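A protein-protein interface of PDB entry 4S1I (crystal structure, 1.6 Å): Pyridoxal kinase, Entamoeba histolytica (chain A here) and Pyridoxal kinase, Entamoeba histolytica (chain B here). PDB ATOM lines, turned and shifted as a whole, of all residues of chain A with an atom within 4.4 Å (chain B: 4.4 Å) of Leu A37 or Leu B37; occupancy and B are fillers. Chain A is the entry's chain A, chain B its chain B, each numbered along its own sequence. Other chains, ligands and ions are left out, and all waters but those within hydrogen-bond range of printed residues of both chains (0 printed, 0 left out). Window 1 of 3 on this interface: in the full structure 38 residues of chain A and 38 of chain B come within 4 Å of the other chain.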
ATOM      1  N   SER A   9     -33.668  -8.954  13.877  1.00  0.00           N
ATOM      2  CA  SER A   9     -33.487  -9.004  12.446  1.00  0.00           C
ATOM      3  C   SER A   9     -33.103 -10.414  12.008  1.00  0.00           C
ATOM      4  O   SER A   9     -32.998 -11.310  12.848  1.00  0.00           O
ATOM      5  CB  SER A   9     -32.456  -7.940  12.019  1.00  0.00           C
ATOM      6  OG  SER A   9     -32.520  -7.744  10.588  1.00  0.00           O
ATOM      7  N   TYR A  11     -31.065 -13.751  10.273  1.00  0.00           N
ATOM      8  CA  TYR A  11     -29.794 -14.441  10.447  1.00  0.00           C
ATOM      9  C   TYR A  11     -29.536 -15.332   9.263  1.00  0.00           C
ATOM     10  O   TYR A  11     -30.460 -16.089   8.822  1.00  0.00           O
ATOM     11  CB  TYR A  11     -29.848 -15.256  11.746  1.00  0.00           C
ATOM     12  CG  TYR A  11     -28.554 -16.065  11.966  1.00  0.00           C
ATOM     13  CD1 TYR A  11     -27.470 -15.464  12.571  1.00  0.00           C
ATOM     14  CD2 TYR A  11     -28.358 -17.278  11.438  1.00  0.00           C
ATOM     15  CE1 TYR A  11     -26.315 -16.151  12.771  1.00  0.00           C
ATOM     16  CE2 TYR A  11     -27.223 -17.992  11.648  1.00  0.00           C
ATOM     17  CZ  TYR A  11     -26.175 -17.405  12.266  1.00  0.00           C
ATOM     18  OH  TYR A  11     -25.002 -18.097  12.420  1.00  0.00           O
ATOM     19  N   ASN A  19     -29.050  -9.302  11.131  1.00  0.00           N
ATOM     20  CA  ASN A  19     -28.427  -9.386  12.454  1.00  0.00           C
ATOM     21  C   ASN A  19     -27.026  -9.956  12.400  1.00  0.00           C
ATOM     22  O   ASN A  19     -26.221  -9.786  13.343  1.00  0.00           O
ATOM     23  CB  ASN A  19     -29.248 -10.160  13.512  1.00  0.00           C
ATOM     24  CG  ASN A  19     -29.941  -9.263  14.482  1.00  0.00           C
ATOM     25  OD1 ASN A  19     -29.603  -8.086  14.630  1.00  0.00           O
ATOM     26  ND2 ASN A  19     -30.842  -9.859  15.296  1.00  0.00           N
ATOM     27  N   MET A  23     -24.130  -8.242  14.427  1.00  0.00           N
ATOM     28  CA  MET A  23     -23.270  -8.899  15.361  1.00  0.00           C
ATOM     29  C   MET A  23     -21.840  -8.474  15.182  1.00  0.00           C
ATOM     30  O   MET A  23     -21.156  -8.120  16.117  1.00  0.00           O
ATOM     31  CB  MET A  23     -23.409 -10.462  15.321  1.00  0.00           C
ATOM     32  CG  MET A  23     -24.768 -11.036  15.779  1.00  0.00           C
ATOM     33  SD  MET A  23     -24.949 -12.828  15.265  1.00  0.00           S
ATOM     34  CE  MET A  23     -26.693 -13.026  15.418  1.00  0.00           C
ATOM     35  N   PHE A  35     -29.187 -10.224  20.417  1.00  0.00           N
ATOM     36  CA  PHE A  35     -29.566 -10.526  19.028  1.00  0.00           C
ATOM     37  C   PHE A  35     -30.663 -11.558  18.914  1.00  0.00           C
ATOM     38  O   PHE A  35     -30.399 -12.775  19.008  1.00  0.00           O
ATOM     39  CB  PHE A  35     -28.319 -10.987  18.271  1.00  0.00           C
ATOM     40  CG  PHE A  35     -27.221  -9.982  18.254  1.00  0.00           C
ATOM     41  CD1 PHE A  35     -27.155  -9.021  17.233  1.00  0.00           C
ATOM     42  CD2 PHE A  35     -26.211  -9.929  19.239  1.00  0.00           C
ATOM     43  CE1 PHE A  35     -26.135  -8.057  17.268  1.00  0.00           C
ATOM     44  CE2 PHE A  35     -25.216  -8.974  19.240  1.00  0.00           C
ATOM     45  CZ  PHE A  35     -25.183  -8.081  18.226  1.00  0.00           C
ATOM     46  N   VAL A  36     -31.881 -11.076  18.697  1.00  0.00           N
ATOM     47  CA  VAL A  36     -33.064 -11.978  18.560  1.00  0.00           C
ATOM     48  C   VAL A  36     -33.246 -12.151  17.033  1.00  0.00           C
ATOM     49  O   VAL A  36     -33.288 -11.197  16.262  1.00  0.00           O
ATOM     50  CB  VAL A  36     -34.344 -11.393  19.119  1.00  0.00           C
ATOM     51  CG1 VAL A  36     -35.505 -12.299  18.836  1.00  0.00           C
ATOM     52  CG2 VAL A  36     -34.222 -11.213  20.623  1.00  0.00           C
ATOM     53  N   LEU A  37     -33.246 -13.385  16.611  1.00  0.00           N
ATOM     54  CA  LEU A  37     -33.277 -13.709  15.173  1.00  0.00           C
ATOM     55  C   LEU A  37     -34.678 -13.850  14.615  1.00  0.00           C
ATOM     56  O   LEU A  37     -35.596 -14.283  15.319  1.00  0.00           O
ATOM     57  CB  LEU A  37     -32.540 -15.014  14.943  1.00  0.00           C
ATOM     58  CG  LEU A  37     -31.152 -15.093  15.542  1.00  0.00           C
ATOM     59  CD1 LEU A  37     -30.464 -16.383  15.180  1.00  0.00           C
ATOM     60  CD2 LEU A  37     -30.259 -13.872  15.341  1.00  0.00           C
ATOM     61  N   THR A  38     -34.885 -13.401  13.411  1.00  0.00           N
ATOM     62  CA  THR A  38     -36.207 -13.526  12.744  1.00  0.00           C
ATOM     63  C   THR A  38     -36.224 -14.607  11.685  1.00  0.00           C
ATOM     64  O   THR A  38     -37.284 -14.976  11.167  1.00  0.00           O
ATOM     65  CB  THR A  38     -36.683 -12.223  12.074  1.00  0.00           C
ATOM     66  OG1 THR A  38     -35.736 -11.881  11.060  1.00  0.00           O
ATOM     67  CG2 THR A  38     -36.812 -11.093  13.127  1.00  0.00           C
ATOM     68  N   THR A  39     -35.016 -15.124  11.368  1.00  0.00           N
ATOM     69  CA  THR A  39     -34.825 -16.208  10.443  1.00  0.00           C
ATOM     70  C   THR A  39     -33.623 -17.014  10.839  1.00  0.00           C
ATOM     71  O   THR A  39     -32.782 -16.554  11.600  1.00  0.00           O
ATOM     72  CB  THR A  39     -34.536 -15.738   8.989  1.00  0.00           C
ATOM     73  OG1 THR A  39     -33.220 -15.175   8.915  1.00  0.00           O
ATOM     74  CG2 THR A  39     -35.529 -14.754   8.455  1.00  0.00           C
ATOM     75  N   HIS A  40     -33.583 -18.248  10.339  1.00  0.00           N
ATOM     76  CA  HIS A  40     -32.370 -19.073  10.445  1.00  0.00           C
ATOM     77  C   HIS A  40     -32.160 -19.675   9.081  1.00  0.00           C
ATOM     78  O   HIS A  40     -32.667 -20.776   8.781  1.00  0.00           O
ATOM     79  CB  HIS A  40     -32.419 -20.089  11.539  1.00  0.00           C
ATOM     80  CG  HIS A  40     -31.247 -21.013  11.685  1.00  0.00           C
ATOM     81  ND1 HIS A  40     -31.382 -22.325  12.123  1.00  0.00           N
ATOM     82  CD2 HIS A  40     -29.937 -20.850  11.424  1.00  0.00           C
ATOM     83  CE1 HIS A  40     -30.177 -22.893  12.172  1.00  0.00           C
ATOM     84  NE2 HIS A  40     -29.280 -21.999  11.776  1.00  0.00           N
ATOM     85  N   VAL A  55     -38.390 -17.645  11.668  1.00  0.00           N
ATOM     86  CA  VAL A  55     -38.691 -17.953  13.070  1.00  0.00           C
ATOM     87  C   VAL A  55     -40.235 -17.886  13.261  1.00  0.00           C
ATOM     88  O   VAL A  55     -40.959 -16.991  12.762  1.00  0.00           O
ATOM     89  CB  VAL A  55     -37.955 -16.964  13.930  1.00  0.00           C
ATOM     90  CG1 VAL A  55     -38.420 -16.992  15.339  1.00  0.00           C
ATOM     91  CG2 VAL A  55     -36.478 -17.253  13.854  1.00  0.00           C
ATOM     92  N   SER B   9     -23.268 -25.578  16.420  1.00  0.00           N
ATOM     93  CA  SER B   9     -23.440 -25.503  17.854  1.00  0.00           C
ATOM     94  C   SER B   9     -24.595 -24.584  18.209  1.00  0.00           C
ATOM     95  O   SER B   9     -25.300 -24.063  17.296  1.00  0.00           O
ATOM     96  CB  SER B   9     -22.134 -25.064  18.543  1.00  0.00           C
ATOM     97  OG  SER B   9     -22.182 -25.348  19.938  1.00  0.00           O
ATOM     98  N   TYR B  11     -27.046 -21.570  19.886  1.00  0.00           N
ATOM     99  CA  TYR B  11     -27.129 -20.117  19.831  1.00  0.00           C
ATOM    100  C   TYR B  11     -28.000 -19.565  20.917  1.00  0.00           C
ATOM    101  O   TYR B  11     -29.141 -20.131  21.205  1.00  0.00           O
ATOM    102  CB  TYR B  11     -27.703 -19.638  18.487  1.00  0.00           C
ATOM    103  CG  TYR B  11     -27.791 -18.154  18.362  1.00  0.00           C
ATOM    104  CD1 TYR B  11     -26.733 -17.375  17.970  1.00  0.00           C
ATOM    105  CD2 TYR B  11     -28.951 -17.496  18.709  1.00  0.00           C
ATOM    106  CE1 TYR B  11     -26.878 -16.013  17.879  1.00  0.00           C
ATOM    107  CE2 TYR B  11     -29.096 -16.141  18.661  1.00  0.00           C
ATOM    108  CZ  TYR B  11     -28.010 -15.365  18.307  1.00  0.00           C
ATOM    109  OH  TYR B  11     -28.156 -13.987  18.247  1.00  0.00           O
ATOM    110  N   ASN B  19     -22.143 -21.445  19.684  1.00  0.00           N
ATOM    111  CA  ASN B  19     -21.778 -20.752  18.420  1.00  0.00           C
ATOM    112  C   ASN B  19     -21.740 -19.250  18.642  1.00  0.00           C
ATOM    113  O   ASN B  19     -21.097 -18.537  17.856  1.00  0.00           O
ATOM    114  CB  ASN B  19     -22.655 -21.104  17.213  1.00  0.00           C
ATOM    115  CG  ASN B  19     -21.978 -21.982  16.248  1.00  0.00           C
ATOM    116  OD1 ASN B  19     -20.733 -22.186  16.301  1.00  0.00           O
ATOM    117  ND2 ASN B  19     -22.712 -22.438  15.300  1.00  0.00           N
ATOM    118  N   MET B  23     -18.760 -17.184  17.164  1.00  0.00           N
ATOM    119  CA  MET B  23     -18.876 -16.037  16.313  1.00  0.00           C
ATOM    120  C   MET B  23     -17.946 -14.879  16.787  1.00  0.00           C
ATOM    121  O   MET B  23     -17.186 -14.324  15.977  1.00  0.00           O
ATOM    122  CB  MET B  23     -20.296 -15.507  16.148  1.00  0.00           C
ATOM    123  CG  MET B  23     -21.310 -16.438  15.535  1.00  0.00           C
ATOM    124  SD  MET B  23     -23.067 -15.946  15.892  1.00  0.00           S
ATOM    125  CE  MET B  23     -23.900 -17.450  15.460  1.00  0.00           C
ATOM    126  N   PHE B  35     -21.726 -20.473  10.394  1.00  0.00           N
ATOM    127  CA  PHE B  35     -22.264 -20.804  11.712  1.00  0.00           C
ATOM    128  C   PHE B  35     -23.679 -21.353  11.575  1.00  0.00           C
ATOM    129  O   PHE B  35     -24.705 -20.592  11.447  1.00  0.00           O
ATOM    130  CB  PHE B  35     -22.294 -19.542  12.618  1.00  0.00           C
ATOM    131  CG  PHE B  35     -20.998 -18.902  12.881  1.00  0.00           C
ATOM    132  CD1 PHE B  35     -20.458 -17.952  11.961  1.00  0.00           C
ATOM    133  CD2 PHE B  35     -20.201 -19.340  13.939  1.00  0.00           C
ATOM    134  CE1 PHE B  35     -19.228 -17.355  12.266  1.00  0.00           C
ATOM    135  CE2 PHE B  35     -18.923 -18.784  14.088  1.00  0.00           C
ATOM    136  CZ  PHE B  35     -18.447 -17.870  13.262  1.00  0.00           C
ATOM    137  N   VAL B  36     -23.784 -22.678  11.635  1.00  0.00           N
ATOM    138  CA  VAL B  36     -25.084 -23.344  11.585  1.00  0.00           C
ATOM    139  C   VAL B  36     -25.541 -23.576  13.024  1.00  0.00           C
ATOM    140  O   VAL B  36     -24.787 -24.113  13.857  1.00  0.00           O
ATOM    141  CB  VAL B  36     -24.997 -24.713  10.867  1.00  0.00           C
ATOM    142  CG1 VAL B  36     -26.318 -25.364  10.887  1.00  0.00           C
ATOM    143  CG2 VAL B  36     -24.552 -24.498   9.428  1.00  0.00           C
ATOM    144  N   LEU B  37     -26.727 -23.101  13.337  1.00  0.00           N
ATOM    145  CA  LEU B  37     -27.245 -23.132  14.703  1.00  0.00           C
ATOM    146  C   LEU B  37     -27.972 -24.430  15.000  1.00  0.00           C
ATOM    147  O   LEU B  37     -28.634 -24.963  14.180  1.00  0.00           O
ATOM    148  CB  LEU B  37     -28.133 -21.916  14.996  1.00  0.00           C
ATOM    149  CG  LEU B  37     -27.524 -20.570  14.554  1.00  0.00           C
ATOM    150  CD1 LEU B  37     -28.507 -19.459  14.898  1.00  0.00           C
ATOM    151  CD2 LEU B  37     -26.076 -20.287  15.000  1.00  0.00           C
ATOM    152  N   THR B  38     -27.866 -24.871  16.247  1.00  0.00           N
ATOM    153  CA  THR B  38     -28.625 -26.050  16.698  1.00  0.00           C
ATOM    154  C   THR B  38     -29.705 -25.690  17.683  1.00  0.00           C
ATOM    155  O   THR B  38     -30.557 -26.521  17.957  1.00  0.00           O
ATOM    156  CB  THR B  38     -27.682 -27.074  17.435  1.00  0.00           C
ATOM    157  OG1 THR B  38     -27.153 -26.429  18.623  1.00  0.00           O
ATOM    158  CG2 THR B  38     -26.539 -27.555  16.539  1.00  0.00           C
ATOM    159  N   THR B  39     -29.713 -24.459  18.090  1.00  0.00           N
ATOM    160  CA  THR B  39     -30.795 -23.880  18.923  1.00  0.00           C
ATOM    161  C   THR B  39     -31.001 -22.441  18.577  1.00  0.00           C
ATOM    162  O   THR B  39     -30.098 -21.771  18.069  1.00  0.00           O
ATOM    163  CB  THR B  39     -30.457 -23.937  20.455  1.00  0.00           C
ATOM    164  OG1 THR B  39     -29.426 -22.957  20.796  1.00  0.00           O
ATOM    165  CG2 THR B  39     -30.012 -25.264  20.915  1.00  0.00           C
ATOM    166  N   HIS B  40     -32.132 -21.903  18.975  1.00  0.00           N
ATOM    167  CA  HIS B  40     -32.345 -20.447  19.005  1.00  0.00           C
ATOM    168  C   HIS B  40     -33.049 -20.102  20.330  1.00  0.00           C
ATOM    169  O   HIS B  40     -34.239 -20.155  20.464  1.00  0.00           O
ATOM    170  CB  HIS B  40     -33.148 -19.962  17.807  1.00  0.00           C
ATOM    171  CG  HIS B  40     -33.466 -18.486  17.797  1.00  0.00           C
ATOM    172  ND1 HIS B  40     -34.591 -18.001  17.171  1.00  0.00           N
ATOM    173  CD2 HIS B  40     -32.803 -17.393  18.267  1.00  0.00           C
ATOM    174  CE1 HIS B  40     -34.619 -16.682  17.309  1.00  0.00           C
ATOM    175  NE2 HIS B  40     -33.527 -16.292  17.930  1.00  0.00           N
ATOM    176  N   VAL B  55     -33.345 -26.404  17.056  1.00  0.00           N
ATOM    177  CA  VAL B  55     -33.541 -26.412  15.605  1.00  0.00           C
ATOM    178  C   VAL B  55     -34.053 -27.770  15.136  1.00  0.00           C
ATOM    179  O   VAL B  55     -33.599 -28.819  15.625  1.00  0.00           O
ATOM    180  CB  VAL B  55     -32.225 -26.059  14.923  1.00  0.00           C
ATOM    181  CG1 VAL B  55     -32.253 -26.297  13.423  1.00  0.00           C
ATOM    182  CG2 VAL B  55     -31.873 -24.618  15.190  1.00  0.00           C
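The side-chain hydroxyl (OH) of Tyr A11 is in hydrogen-bond range of the backbone carbonyl oxygen (O) of Phe B35. O of Phe A35 lies within hydrogen-bond range of OH of Tyr B11 (2.7 Å). A ring nitrogen (NE2) of His B40 sits at hydrogen-bond distance from the backbone NH (N) of Leu A37 (3.2 Å). N of Leu B37 is in hydrogen-bond range of NE2 of His A40, at 3.2 Å. SD of Met B23 lies close to SD of Met A23, at 3.7 Å.
Among the printed residues, merely in contact across the chains: Tyr A11 with Met B23, Met A23 with Tyr B11, Tyr A11 with Leu B37, Leu A37 with Tyr B11, Leu A37 with Leu B37, His A40 with Val B55 and Val A55 with His B40.
Of chain B, only Tyr B11 (3.6 Å), Leu B37 (3.7 Å) and His B40 (3.2 Å) come within 4 Å of Leu A37. Leu B37 touches just these residues of chain A: Tyr A11 (3.6 Å), Leu A37 (3.7 Å) and His A40 (3.2 Å). Of the printed residues of chain A, Phe B35 touches Tyr A11 (2.7 Å). Of the printed residues of chain B, Tyr A11 touches Met B23 (3.3 Å), Phe B35 (2.7 Å) and Leu B37 (3.6 Å). Thr B39 touches none of the printed residues of chain A. Thr A39 touches none of the printed residues of chain B. The nearest printed residue of chain B that does not touch Leu A37 is Thr B39 (6.1 Å). The nearest printed residue of chain A that does not touch Leu B37 is Thr A39 (6.1 Å). The nearest printed residue of chain B that does not touch Tyr A11 is Val B36 (4.8 Å).
Of the 11 printed residues of chain B, 6 touch a printed residue of chain A. Hydrophobic or aromatic side chains of chain A that line the printed part of chain B: Tyr A11, Met A23, Phe A35, Leu A37, His A40 and Val A55. Among the printed residues, 12 pairs touch across the chains.
The backbone carbonyl oxygen (O) of Tyr A11 lies within hydrogen-bond range of the side-chain hydroxyl (OG1) of Thr A39 (2.9 Å). The backbone NH (N) of Val A55 sits at hydrogen-bond distance from the backbone carbonyl oxygen (O) of Thr A38, at 2.9 Å. The backbone carbonyl oxygen (O) of Tyr B11 is in hydrogen-bond range of the side-chain hydroxyl (OG1) of Thr B39, at 2.9 Å. The backbone carbonyl oxygen of Thr B38 sits at hydrogen-bond distance from the backbone NH of Val B55, at 2.9 Å.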
